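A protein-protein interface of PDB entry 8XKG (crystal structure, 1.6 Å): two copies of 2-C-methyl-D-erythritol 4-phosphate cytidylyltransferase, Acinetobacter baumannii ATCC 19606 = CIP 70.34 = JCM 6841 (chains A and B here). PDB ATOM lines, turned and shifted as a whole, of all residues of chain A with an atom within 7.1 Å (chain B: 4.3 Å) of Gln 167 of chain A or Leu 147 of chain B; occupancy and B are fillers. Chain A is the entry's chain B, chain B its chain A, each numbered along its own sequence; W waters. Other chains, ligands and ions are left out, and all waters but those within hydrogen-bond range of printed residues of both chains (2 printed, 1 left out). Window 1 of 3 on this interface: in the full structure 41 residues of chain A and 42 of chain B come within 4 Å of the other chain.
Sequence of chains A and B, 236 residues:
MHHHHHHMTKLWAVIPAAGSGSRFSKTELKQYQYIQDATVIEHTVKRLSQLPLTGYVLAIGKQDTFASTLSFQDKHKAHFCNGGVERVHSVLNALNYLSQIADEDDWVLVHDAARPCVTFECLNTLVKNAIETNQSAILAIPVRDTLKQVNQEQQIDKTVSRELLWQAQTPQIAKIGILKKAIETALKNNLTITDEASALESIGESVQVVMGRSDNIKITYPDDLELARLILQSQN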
ATOM      1  N   ARG A 115       3.287 -13.343   7.150  1.00  0.00           N
ATOM      2  CA  ARG A 115       1.869 -13.282   7.503  1.00  0.00           C
ATOM      3  C   ARG A 115       1.336 -14.667   7.134  1.00  0.00           C
ATOM      4  O   ARG A 115       0.875 -14.885   6.006  1.00  0.00           O
ATOM      5  CB  ARG A 115       1.151 -12.157   6.758  1.00  0.00           C
ATOM      6  CG  ARG A 115       1.454 -10.748   7.269  1.00  0.00           C
ATOM      7  CD  ARG A 115       0.531  -9.717   6.617  1.00  0.00           C
ATOM      8  NE  ARG A 115       1.033  -8.352   6.744  1.00  0.00           N
ATOM      9  CZ  ARG A 115       0.558  -7.449   7.593  1.00  0.00           C
ATOM     10  NH1 ARG A 115      -0.433  -7.732   8.422  1.00  0.00           N
ATOM     11  NH2 ARG A 115       1.094  -6.232   7.612  1.00  0.00           N
ATOM     12  N   ILE A 138      -6.477  -4.135  -1.370  1.00  0.00           N
ATOM     13  CA  ILE A 138      -5.632  -4.687  -0.318  1.00  0.00           C
ATOM     14  C   ILE A 138      -6.503  -5.073   0.868  1.00  0.00           C
ATOM     15  O   ILE A 138      -7.582  -4.513   1.082  1.00  0.00           O
ATOM     16  CB  ILE A 138      -4.531  -3.701   0.144  1.00  0.00           C
ATOM     17  CG1 ILE A 138      -5.127  -2.609   1.036  1.00  0.00           C
ATOM     18  CG2 ILE A 138      -3.809  -3.087  -1.047  1.00  0.00           C
ATOM     19  CD1 ILE A 138      -4.098  -1.737   1.716  1.00  0.00           C
ATOM     20  N   LEU A 139      -6.022  -6.035   1.651  1.00  0.00           N
ATOM     21  CA  LEU A 139      -6.572  -6.244   2.980  1.00  0.00           C
ATOM     22  C   LEU A 139      -6.046  -5.162   3.912  1.00  0.00           C
ATOM     23  O   LEU A 139      -4.876  -4.774   3.836  1.00  0.00           O
ATOM     24  CB  LEU A 139      -6.212  -7.623   3.532  1.00  0.00           C
ATOM     25  CG  LEU A 139      -6.811  -8.862   2.868  1.00  0.00           C
ATOM     26  CD1 LEU A 139      -6.332 -10.112   3.591  1.00  0.00           C
ATOM     27  CD2 LEU A 139      -8.331  -8.796   2.833  1.00  0.00           C
ATOM     28  N   ALA A 140      -6.923  -4.667   4.781  1.00  0.00           N
ATOM     29  CA  ALA A 140      -6.555  -3.643   5.748  1.00  0.00           C
ATOM     30  C   ALA A 140      -7.552  -3.681   6.895  1.00  0.00           C
ATOM     31  O   ALA A 140      -8.671  -4.179   6.750  1.00  0.00           O
ATOM     32  CB  ALA A 140      -6.523  -2.251   5.106  1.00  0.00           C
ATOM     33  N   ILE A 141      -7.137  -3.145   8.038  1.00  0.00           N
ATOM     34  CA  ILE A 141      -8.053  -3.012   9.169  1.00  0.00           C
ATOM     35  C   ILE A 141      -7.982  -1.586   9.700  1.00  0.00           C
ATOM     36  O   ILE A 141      -6.918  -0.954   9.634  1.00  0.00           O
ATOM     37  CB  ILE A 141      -7.742  -4.028  10.282  1.00  0.00           C
ATOM     38  CG1 ILE A 141      -6.310  -3.862  10.799  1.00  0.00           C
ATOM     39  CG2 ILE A 141      -7.967  -5.447   9.792  1.00  0.00           C
ATOM     40  CD1 ILE A 141      -5.978  -4.789  11.951  1.00  0.00           C
ATOM     41  N   PRO A 142      -9.078  -1.039  10.223  1.00  0.00           N
ATOM     42  CA  PRO A 142      -9.017   0.308  10.799  1.00  0.00           C
ATOM     43  C   PRO A 142      -8.101   0.331  12.011  1.00  0.00           C
ATOM     44  O   PRO A 142      -7.991  -0.648  12.753  1.00  0.00           O
ATOM     45  CB  PRO A 142     -10.470   0.610  11.187  1.00  0.00           C
ATOM     46  CG  PRO A 142     -11.305  -0.445  10.556  1.00  0.00           C
ATOM     47  CD  PRO A 142     -10.435  -1.609  10.232  1.00  0.00           C
ATOM     48  N   VAL A 143      -7.437   1.467  12.207  1.00  0.00           N
ATOM     49  CA  VAL A 143      -6.633   1.662  13.408  1.00  0.00           C
ATOM     50  C   VAL A 143      -7.570   1.773  14.603  1.00  0.00           C
ATOM     51  O   VAL A 143      -8.456   2.636  14.638  1.00  0.00           O
ATOM     52  CB  VAL A 143      -5.743   2.905  13.281  1.00  0.00           C
ATOM     53  CG1 VAL A 143      -5.020   3.178  14.595  1.00  0.00           C
ATOM     54  CG2 VAL A 143      -4.760   2.744  12.130  1.00  0.00           C
ATOM     55  N   ARG A 144      -7.385   0.893  15.587  1.00  0.00           N
ATOM     56  CA  ARG A 144      -8.214   0.885  16.783  1.00  0.00           C
ATOM     57  C   ARG A 144      -7.490   1.372  18.029  1.00  0.00           C
ATOM     58  O   ARG A 144      -8.150   1.822  18.970  1.00  0.00           O
ATOM     59  CB  ARG A 144      -8.748  -0.530  17.049  1.00  0.00           C
ATOM     60  CG  ARG A 144      -9.771  -1.028  16.037  1.00  0.00           C
ATOM     61  CD  ARG A 144     -11.106  -0.310  16.167  1.00  0.00           C
ATOM     62  NE  ARG A 144     -11.816  -0.683  17.385  1.00  0.00           N
ATOM     63  CZ  ARG A 144     -12.799  -1.572  17.442  1.00  0.00           C
ATOM     64  NH1 ARG A 144     -13.202  -2.229  16.366  1.00  0.00           N
ATOM     65  NH2 ARG A 144     -13.393  -1.807  18.609  1.00  0.00           N
ATOM     66  N   ASP A 145      -6.164   1.299  18.052  1.00  0.00           N
ATOM     67  CA  ASP A 145      -5.375   1.745  19.187  1.00  0.00           C
ATOM     68  C   ASP A 145      -5.091   3.234  19.048  1.00  0.00           C
ATOM     69  O   ASP A 145      -5.007   3.767  17.939  1.00  0.00           O
ATOM     70  CB  ASP A 145      -4.055   0.975  19.266  1.00  0.00           C
ATOM     71  CG  ASP A 145      -4.241  -0.470  19.683  1.00  0.00           C
ATOM     72  OD1 ASP A 145      -5.300  -0.809  20.253  1.00  0.00           O
ATOM     73  OD2 ASP A 145      -3.312  -1.275  19.451  1.00  0.00           O
ATOM     74  N   LEU A 147      -2.800   6.275  18.775  1.00  0.00           N
ATOM     75  CA  LEU A 147      -1.458   6.391  18.221  1.00  0.00           C
ATOM     76  C   LEU A 147      -0.665   7.474  18.935  1.00  0.00           C
ATOM     77  O   LEU A 147      -1.182   8.557  19.220  1.00  0.00           O
ATOM     78  CB  LEU A 147      -1.505   6.704  16.727  1.00  0.00           C
ATOM     79  CG  LEU A 147      -2.214   5.682  15.850  1.00  0.00           C
ATOM     80  CD1 LEU A 147      -2.132   6.131  14.409  1.00  0.00           C
ATOM     81  CD2 LEU A 147      -1.599   4.306  16.036  1.00  0.00           C
ATOM     82  N   VAL A 160      -1.495  11.112  17.982  1.00  0.00           N
ATOM     83  CA  VAL A 160      -1.750  11.305  16.558  1.00  0.00           C
ATOM     84  C   VAL A 160      -3.136  10.760  16.221  1.00  0.00           C
ATOM     85  O   VAL A 160      -3.528   9.692  16.704  1.00  0.00           O
ATOM     86  CB  VAL A 160      -0.651  10.622  15.715  1.00  0.00           C
ATOM     87  CG1 VAL A 160      -1.031  10.575  14.242  1.00  0.00           C
ATOM     88  CG2 VAL A 160       0.699  11.311  15.925  1.00  0.00           C
ATOM     89  N   LEU A 165      -7.574   6.359   9.246  1.00  0.00           N
ATOM     90  CA  LEU A 165      -6.365   5.570   9.133  1.00  0.00           C
ATOM     91  C   LEU A 165      -6.685   4.089   9.236  1.00  0.00           C
ATOM     92  O   LEU A 165      -7.423   3.657  10.128  1.00  0.00           O
ATOM     93  CB  LEU A 165      -5.367   5.966  10.220  1.00  0.00           C
ATOM     94  CG  LEU A 165      -4.773   7.362  10.028  1.00  0.00           C
ATOM     95  CD1 LEU A 165      -3.398   7.464  10.664  1.00  0.00           C
ATOM     96  CD2 LEU A 165      -4.721   7.747   8.551  1.00  0.00           C
ATOM     97  N   TRP A 166      -6.107   3.321   8.325  1.00  0.00           N
ATOM     98  CA  TRP A 166      -6.183   1.874   8.324  1.00  0.00           C
ATOM     99  C   TRP A 166      -4.762   1.340   8.320  1.00  0.00           C
ATOM    100  O   TRP A 166      -3.849   1.966   7.772  1.00  0.00           O
ATOM    101  CB  TRP A 166      -6.950   1.341   7.101  1.00  0.00           C
ATOM    102  CG  TRP A 166      -8.424   1.662   7.073  1.00  0.00           C
ATOM    103  CD1 TRP A 166      -9.006   2.890   7.214  1.00  0.00           C
ATOM    104  CD2 TRP A 166      -9.495   0.735   6.860  1.00  0.00           C
ATOM    105  NE1 TRP A 166     -10.373   2.780   7.118  1.00  0.00           N
ATOM    106  CE2 TRP A 166     -10.699   1.467   6.901  1.00  0.00           C
ATOM    107  CE3 TRP A 166      -9.553  -0.646   6.648  1.00  0.00           C
ATOM    108  CZ2 TRP A 166     -11.945   0.865   6.735  1.00  0.00           C
ATOM    109  CZ3 TRP A 166     -10.791  -1.241   6.484  1.00  0.00           C
ATOM    110  CH2 TRP A 166     -11.969  -0.486   6.529  1.00  0.00           C
ATOM    111  N   GLN A 167      -4.572   0.186   8.946  1.00  0.00           N
ATOM    112  CA  GLN A 167      -3.301  -0.520   8.873  1.00  0.00           C
ATOM    113  C   GLN A 167      -3.356  -1.423   7.651  1.00  0.00           C
ATOM    114  O   GLN A 167      -4.168  -2.351   7.593  1.00  0.00           O
ATOM    115  CB  GLN A 167      -3.046  -1.309  10.153  1.00  0.00           C
ATOM    116  CG  GLN A 167      -3.061  -0.430  11.388  1.00  0.00           C
ATOM    117  CD  GLN A 167      -3.143  -1.207  12.686  1.00  0.00           C
ATOM    118  OE1 GLN A 167      -3.624  -0.690  13.693  1.00  0.00           O
ATOM    119  NE2 GLN A 167      -2.664  -2.446  12.675  1.00  0.00           N
ATOM    120  N   ALA A 168      -2.514  -1.135   6.665  1.00  0.00           N
ATOM    121  CA  ALA A 168      -2.456  -1.984   5.488  1.00  0.00           C
ATOM    122  C   ALA A 168      -1.922  -3.354   5.875  1.00  0.00           C
ATOM    123  O   ALA A 168      -0.968  -3.473   6.648  1.00  0.00           O
ATOM    124  CB  ALA A 168      -1.575  -1.355   4.410  1.00  0.00           C
ATOM    125  N   GLN A 169      -2.561  -4.389   5.355  1.00  0.00           N
ATOM    126  CA  GLN A 169      -2.076  -5.753   5.470  1.00  0.00           C
ATOM    127  C   GLN A 169      -1.831  -6.263   4.053  1.00  0.00           C
ATOM    128  O   GLN A 169      -1.893  -5.507   3.080  1.00  0.00           O
ATOM    129  CB  GLN A 169      -3.099  -6.628   6.199  1.00  0.00           C
ATOM    130  CG  GLN A 169      -3.492  -6.069   7.559  1.00  0.00           C
ATOM    131  CD  GLN A 169      -4.459  -6.956   8.312  1.00  0.00           C
ATOM    132  OE1 GLN A 169      -5.294  -7.637   7.717  1.00  0.00           O
ATOM    133  NE2 GLN A 169      -4.357  -6.947   9.636  1.00  0.00           N
ATOM    134  N   THR A 170      -1.505  -7.542   3.943  1.00  0.00           N
ATOM    135  CA  THR A 170      -1.422  -8.231   2.667  1.00  0.00           C
ATOM    136  C   THR A 170      -2.298  -9.475   2.687  1.00  0.00           C
ATOM    137  O   THR A 170      -2.668  -9.959   3.762  1.00  0.00           O
ATOM    138  CB  THR A 170       0.042  -8.596   2.363  1.00  0.00           C
ATOM    139  OG1 THR A 170       0.441  -9.724   3.147  1.00  0.00           O
ATOM    140  CG2 THR A 170       0.967  -7.424   2.648  1.00  0.00           C
ATOM    141  N   THR A 194       6.550   1.942  -0.565  1.00  0.00           N
ATOM    142  CA  THR A 194       6.495   1.070   0.602  1.00  0.00           C
ATOM    143  C   THR A 194       5.873  -0.270   0.221  1.00  0.00           C
ATOM    144  O   THR A 194       6.540  -1.304   0.241  1.00  0.00           O
ATOM    145  CB  THR A 194       5.675   1.702   1.741  1.00  0.00           C
ATOM    146  OG1 THR A 194       4.573   2.433   1.190  1.00  0.00           O
ATOM    147  CG2 THR A 194       6.544   2.643   2.562  1.00  0.00           C
ATOM    148  N   ASP A 195       4.590  -0.240  -0.126  1.00  0.00           N
ATOM    149  CA  ASP A 195       3.870  -1.442  -0.524  1.00  0.00           C
ATOM    150  C   ASP A 195       3.369  -1.299  -1.956  1.00  0.00           C
ATOM    151  O   ASP A 195       3.626  -0.289  -2.612  1.00  0.00           O
ATOM    152  CB  ASP A 195       2.697  -1.705   0.424  1.00  0.00           C
ATOM    153  CG  ASP A 195       1.782  -0.503   0.565  1.00  0.00           C
ATOM    154  OD1 ASP A 195       2.012   0.507  -0.134  1.00  0.00           O
ATOM    155  OD2 ASP A 195       0.832  -0.570   1.372  1.00  0.00           O
ATOM    156  N   GLY A 212      -9.482  -6.826   6.599  1.00  0.00           N
ATOM    157  CA  GLY A 212      -8.616  -7.898   7.052  1.00  0.00           C
ATOM    158  C   GLY A 212      -9.015  -8.389   8.425  1.00  0.00           C
ATOM    159  O   GLY A 212     -10.193  -8.393   8.794  1.00  0.00           O
ATOM    160  N   SER A 214      -7.479  -8.527  12.710  1.00  0.00           N
ATOM    161  CA  SER A 214      -6.459  -8.168  13.685  1.00  0.00           C
ATOM    162  C   SER A 214      -5.462  -9.301  13.888  1.00  0.00           C
ATOM    163  O   SER A 214      -4.316  -9.051  14.277  1.00  0.00           O
ATOM    164  CB  SER A 214      -7.109  -7.771  15.011  1.00  0.00           C
ATOM    165  OG  SER A 214      -7.951  -8.800  15.498  1.00  0.00           O
ATOM    166  N   VAL B 143       4.219   0.774  15.671  1.00  0.00           N
ATOM    167  CA  VAL B 143       3.395   0.513  14.495  1.00  0.00           C
ATOM    168  C   VAL B 143       4.241  -0.225  13.465  1.00  0.00           C
ATOM    169  O   VAL B 143       5.308   0.253  13.063  1.00  0.00           O
ATOM    170  CB  VAL B 143       2.836   1.821  13.919  1.00  0.00           C
ATOM    171  CG1 VAL B 143       2.174   1.574  12.577  1.00  0.00           C
ATOM    172  CG2 VAL B 143       1.845   2.443  14.885  1.00  0.00           C
ATOM    173  N   ASP B 145       2.561  -1.928  10.575  1.00  0.00           N
ATOM    174  CA  ASP B 145       1.858  -1.906   9.301  1.00  0.00           C
ATOM    175  C   ASP B 145       1.963  -0.534   8.645  1.00  0.00           C
ATOM    176  O   ASP B 145       1.998   0.497   9.322  1.00  0.00           O
ATOM    177  CB  ASP B 145       0.383  -2.253   9.496  1.00  0.00           C
ATOM    178  CG  ASP B 145       0.181  -3.613  10.121  1.00  0.00           C
ATOM    179  OD1 ASP B 145       0.937  -4.543   9.775  1.00  0.00           O
ATOM    180  OD2 ASP B 145      -0.726  -3.747  10.969  1.00  0.00           O
ATOM    181  N   THR B 146       1.978  -0.529   7.314  1.00  0.00           N
ATOM    182  CA  THR B 146       1.910   0.725   6.576  1.00  0.00           C
ATOM    183  C   THR B 146       0.525   1.336   6.764  1.00  0.00           C
ATOM    184  O   THR B 146      -0.489   0.639   6.660  1.00  0.00           O
ATOM    185  CB  THR B 146       2.205   0.491   5.092  1.00  0.00           C
ATOM    186  OG1 THR B 146       3.526  -0.045   4.942  1.00  0.00           O
ATOM    187  CG2 THR B 146       2.115   1.796   4.311  1.00  0.00           C
ATOM    188  N   LEU B 147       0.480   2.629   7.079  1.00  0.00           N
ATOM    189  CA  LEU B 147      -0.778   3.307   7.370  1.00  0.00           C
ATOM    190  C   LEU B 147      -1.335   3.983   6.123  1.00  0.00           C
ATOM    191  O   LEU B 147      -0.599   4.619   5.362  1.00  0.00           O
ATOM    192  CB  LEU B 147      -0.584   4.335   8.486  1.00  0.00           C
ATOM    193  CG  LEU B 147      -0.110   3.776   9.829  1.00  0.00           C
ATOM    194  CD1 LEU B 147       0.142   4.893  10.828  1.00  0.00           C
ATOM    195  CD2 LEU B 147      -1.136   2.802  10.379  1.00  0.00           C
ATOM    196  N   LYS B 148      -2.648   3.850   5.926  1.00  0.00           N
ATOM    197  CA  LYS B 148      -3.343   4.408   4.773  1.00  0.00           C
ATOM    198  C   LYS B 148      -4.491   5.294   5.229  1.00  0.00           C
ATOM    199  O   LYS B 148      -5.271   4.901   6.102  1.00  0.00           O
ATOM    200  CB  LYS B 148      -3.894   3.298   3.871  1.00  0.00           C
ATOM    201  CG  LYS B 148      -2.885   2.250   3.447  1.00  0.00           C
ATOM    202  CD  LYS B 148      -1.837   2.831   2.520  1.00  0.00           C
ATOM    203  CE  LYS B 148      -0.960   1.734   1.949  1.00  0.00           C
ATOM    204  NZ  LYS B 148       0.064   2.266   1.009  1.00  0.00           N
ATOM    205  N   THR B 159      -0.741   7.220   1.433  1.00  0.00           N
ATOM    206  CA  THR B 159       0.010   6.610   2.520  1.00  0.00           C
ATOM    207  C   THR B 159       0.388   7.667   3.550  1.00  0.00           C
ATOM    208  O   THR B 159       0.785   8.782   3.201  1.00  0.00           O
ATOM    209  CB  THR B 159       1.271   5.925   1.984  1.00  0.00           C
ATOM    210  OG1 THR B 159       0.904   4.927   1.022  1.00  0.00           O
ATOM    211  CG2 THR B 159       2.059   5.270   3.110  1.00  0.00           C
ATOM    212  N   VAL B 160       0.252   7.313   4.824  1.00  0.00           N
ATOM    213  CA  VAL B 160       0.559   8.206   5.934  1.00  0.00           C
ATOM    214  C   VAL B 160       1.803   7.678   6.636  1.00  0.00           C
ATOM    215  O   VAL B 160       1.917   6.472   6.886  1.00  0.00           O
ATOM    216  CB  VAL B 160      -0.633   8.308   6.906  1.00  0.00           C
ATOM    217  CG1 VAL B 160      -0.189   8.845   8.257  1.00  0.00           C
ATOM    218  CG2 VAL B 160      -1.745   9.159   6.304  1.00  0.00           C
ATOM    219  N   SER B 161       2.728   8.580   6.962  1.00  0.00           N
ATOM    220  CA  SER B 161       3.974   8.171   7.598  1.00  0.00           C
ATOM    221  C   SER B 161       3.705   7.488   8.933  1.00  0.00           C
ATOM    222  O   SER B 161       2.846   7.914   9.709  1.00  0.00           O
ATOM    223  CB  SER B 161       4.883   9.382   7.815  1.00  0.00           C
ATOM    224  OG  SER B 161       6.057   9.011   8.518  1.00  0.00           O
ATOM    225  N   ARG B 162       4.460   6.425   9.203  1.00  0.00           N
ATOM    226  CA  ARG B 162       4.410   5.730  10.481  1.00  0.00           C
ATOM    227  C   ARG B 162       5.693   5.930  11.272  1.00  0.00           C
ATOM    228  O   ARG B 162       5.885   5.290  12.310  1.00  0.00           O
ATOM    229  CB  ARG B 162       4.117   4.240  10.291  1.00  0.00           C
ATOM    230  CG  ARG B 162       5.255   3.406   9.746  1.00  0.00           C
ATOM    231  CD  ARG B 162       4.779   1.982   9.517  1.00  0.00           C
ATOM    232  NE  ARG B 162       5.728   1.205   8.732  1.00  0.00           N
ATOM    233  CZ  ARG B 162       6.719   0.491   9.248  1.00  0.00           C
ATOM    234  NH1 ARG B 162       6.920   0.431  10.553  1.00  0.00           N
ATOM    235  NH2 ARG B 162       7.532  -0.172   8.431  1.00  0.00           N
ATOM    236  N   LEU B 165       5.803   6.258  15.215  1.00  0.00           N
ATOM    237  CA  LEU B 165       4.463   6.019  15.737  1.00  0.00           C
ATOM    238  C   LEU B 165       4.398   4.702  16.501  1.00  0.00           C
ATOM    239  O   LEU B 165       4.959   3.690  16.072  1.00  0.00           O
ATOM    240  CB  LEU B 165       3.427   6.025  14.614  1.00  0.00           C
ATOM    241  CG  LEU B 165       3.232   7.364  13.902  1.00  0.00           C
ATOM    242  CD1 LEU B 165       1.901   7.372  13.170  1.00  0.00           C
ATOM    243  CD2 LEU B 165       3.327   8.529  14.881  1.00  0.00           C
ATOM    244  N   GLN B 167       1.546   2.161  18.875  1.00  0.00           N
ATOM    245  CA  GLN B 167       0.191   1.836  19.312  1.00  0.00           C
ATOM    246  C   GLN B 167       0.151   1.737  20.833  1.00  0.00           C
ATOM    247  O   GLN B 167       0.783   0.849  21.415  1.00  0.00           O
ATOM    248  CB  GLN B 167      -0.280   0.517  18.705  1.00  0.00           C
ATOM    249  CG  GLN B 167      -0.440   0.511  17.208  1.00  0.00           C
ATOM    250  CD  GLN B 167      -0.542  -0.897  16.664  1.00  0.00           C
ATOM    251  OE1 GLN B 167      -1.258  -1.734  17.214  1.00  0.00           O
ATOM    252  NE2 GLN B 167       0.161  -1.162  15.572  1.00  0.00           N
HETATM  253  O   HOH W   1       5.650  -1.681   3.361  1.00  0.00           O
HETATM  254  O   HOH W   2      -2.512  -3.919  15.421  1.00  0.00           O
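The side-chain carboxylate (OD1) of Asp 145 of chain B is in salt-bridge range of the guanidinium group (NH2) of Arg 115 of chain A, 2.7 Å away. The side-chain carboxylate (OD2) of Asp 145 of chain B sits at hydrogen-bond distance from the side-chain amide nitrogen (NE2) of Gln 167 of chain A, 2.9 Å away. The backbone NH (N) of Ala 168 of chain A sits at hydrogen-bond distance from the backbone carbonyl oxygen (O) of Thr 146 of chain B. The backbone carbonyl oxygen (O) of Lys 148 of chain B is in hydrogen-bond range of the backbone NH (N) of Trp 166 of chain A (2.9 Å). The side-chain amino group (NZ) of Lys 148 of chain B lies within salt-bridge range of the side-chain carboxylate (OD1) of Asp 195 of chain A (2.9 Å). The side-chain amide oxygen (OE1) of Gln 167 of chain B lies close to the side-chain carboxylate (OD2) of Asp 145 of chain A, at 3.1 Å.
N of Val 143 of chain B lies within hydrogen-bond range of O of Leu 165 of chain B. The backbone carbonyl oxygen (O) of Leu 147 of chain B lies within hydrogen-bond range of the backbone NH (N) of Val 160 of chain B. The side-chain amino group (NZ) of Lys 148 of chain B is in hydrogen-bond range of the side-chain hydroxyl (OG1) of Thr 159 of chain B (2.8 Å). The backbone carbonyl oxygen of Leu 165 of chain A lies within hydrogen-bond range of the backbone NH of Val 143 of chain A (3.0 Å). The backbone carbonyl oxygen of Leu 147 of chain A is in hydrogen-bond range of the backbone NH of Val 160 of chain A (2.9 Å). The side-chain carboxylate (OD1) of Asp 195 of chain A is in hydrogen-bond range of the side-chain hydroxyl (OG1) of Thr 194 of chain A (3.5 Å).
Val 160 of chain A touches Leu 165 of chain B (CG2 to CD2, 3.97 Å). Leu 165 of chain A touches Lys 148 of chain B. CD2 of Leu 165 of chain A touches CG2 of Val 160 of chain B, at 3.99 Å. O of Trp 166 of chain A touches O of Thr 146 of chain B (3.8 Å). O of Trp 166 of chain A touches CA of Leu 147 of chain B, 3.4 Å away. O of Thr 146 of chain B touches C of Gln 167 of chain A (3.7 Å). CG of Gln 167 of chain A touches CD2 of Leu 147 of chain B, at 3.9 Å. Ala 168 of chain A touches Asp 145 of chain B (O to CB, 3.4 Å). Lys 148 of chain B touches Ala 168 of chain A (CG to CB, 3.95 Å). Thr 146 of chain B touches Asp 195 of chain A (CG2 to OD2, 3.99 Å).
Printed residues of chain B within 4 Å of Gln 167 of chain A: Asp 145, Thr 146 and Leu 147. Leu 147 of chain B touches two residues of chain A. Of the printed residues of chain A, Asp 145 of chain B touches Arg 115 (2.7 Å), Gln 167 (2.9 Å) and Ala 168 (3.4 Å). Printed residues of chain B within 4 Å of Trp 166 of chain A: Thr 146 (3.8 Å), Leu 147 (3.4 Å) and Lys 148 (2.9 Å). Thr 194 of chain A touches none of the printed residues of chain B. Thr 170 of chain A touches none of the printed residues of chain B. The nearest residue of chain B that does not touch Gln 167 of chain A is Gln 167 of chain B (4.2 Å). The nearest residue of chain A that does not touch Leu 147 of chain B is Val 143 of chain A (4.03 Å). The nearest printed residue of chain B that does not touch Val 160 of chain A is Val 160 of chain B (6.3 Å).
Hydrophobic or aromatic side chains of chain A that line the printed part of chain B: Val 160, Leu 165 and Ala 168. Along chain A the printed residues that touch a printed residue of chain B span positions 115 to 195. Hydrophobic or aromatic side chains of chain B that line the printed part of chain A: Leu 147, Val 160 and Leu 165. Among the printed residues, 16 pairs touch across the chains. Among the printed residues, Asp or Glu carboxylates within 4 Å of a Lys or Arg side-chain nitrogen of the other chain: Arg 115 of chain A with Asp 145 of chain B and Asp 195 of chain A with Lys 148 of chain B.
Asp 145 of chain A touches Gln 167 of chain B, and with the chains exchanged Gln 167 of chain A touches Asp 145 of chain B. Val 160 of chain A touches Leu 165 of chain B, and with the chains exchanged Leu 165 of chain A touches Val 160 of chain B. Gln 167 of chain A touches Leu 147 of chain B, but with the chains exchanged Leu 147 of chain A does not touch Gln 167 of chain B (4.1 Å). Positions printed for both chains: 143, 145, 147, 160, 165 and 167.
Water W2 lies within hydrogen-bond range of OE1 of Gln 167 of chain B (3.1 Å) and NE2 of Gln 167 of chain A (3.1 Å). Water W1 lies within hydrogen-bond range of OG1 of Thr 146 of chain B (3.1 Å) and O of Thr 194 of chain A (3.3 Å).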
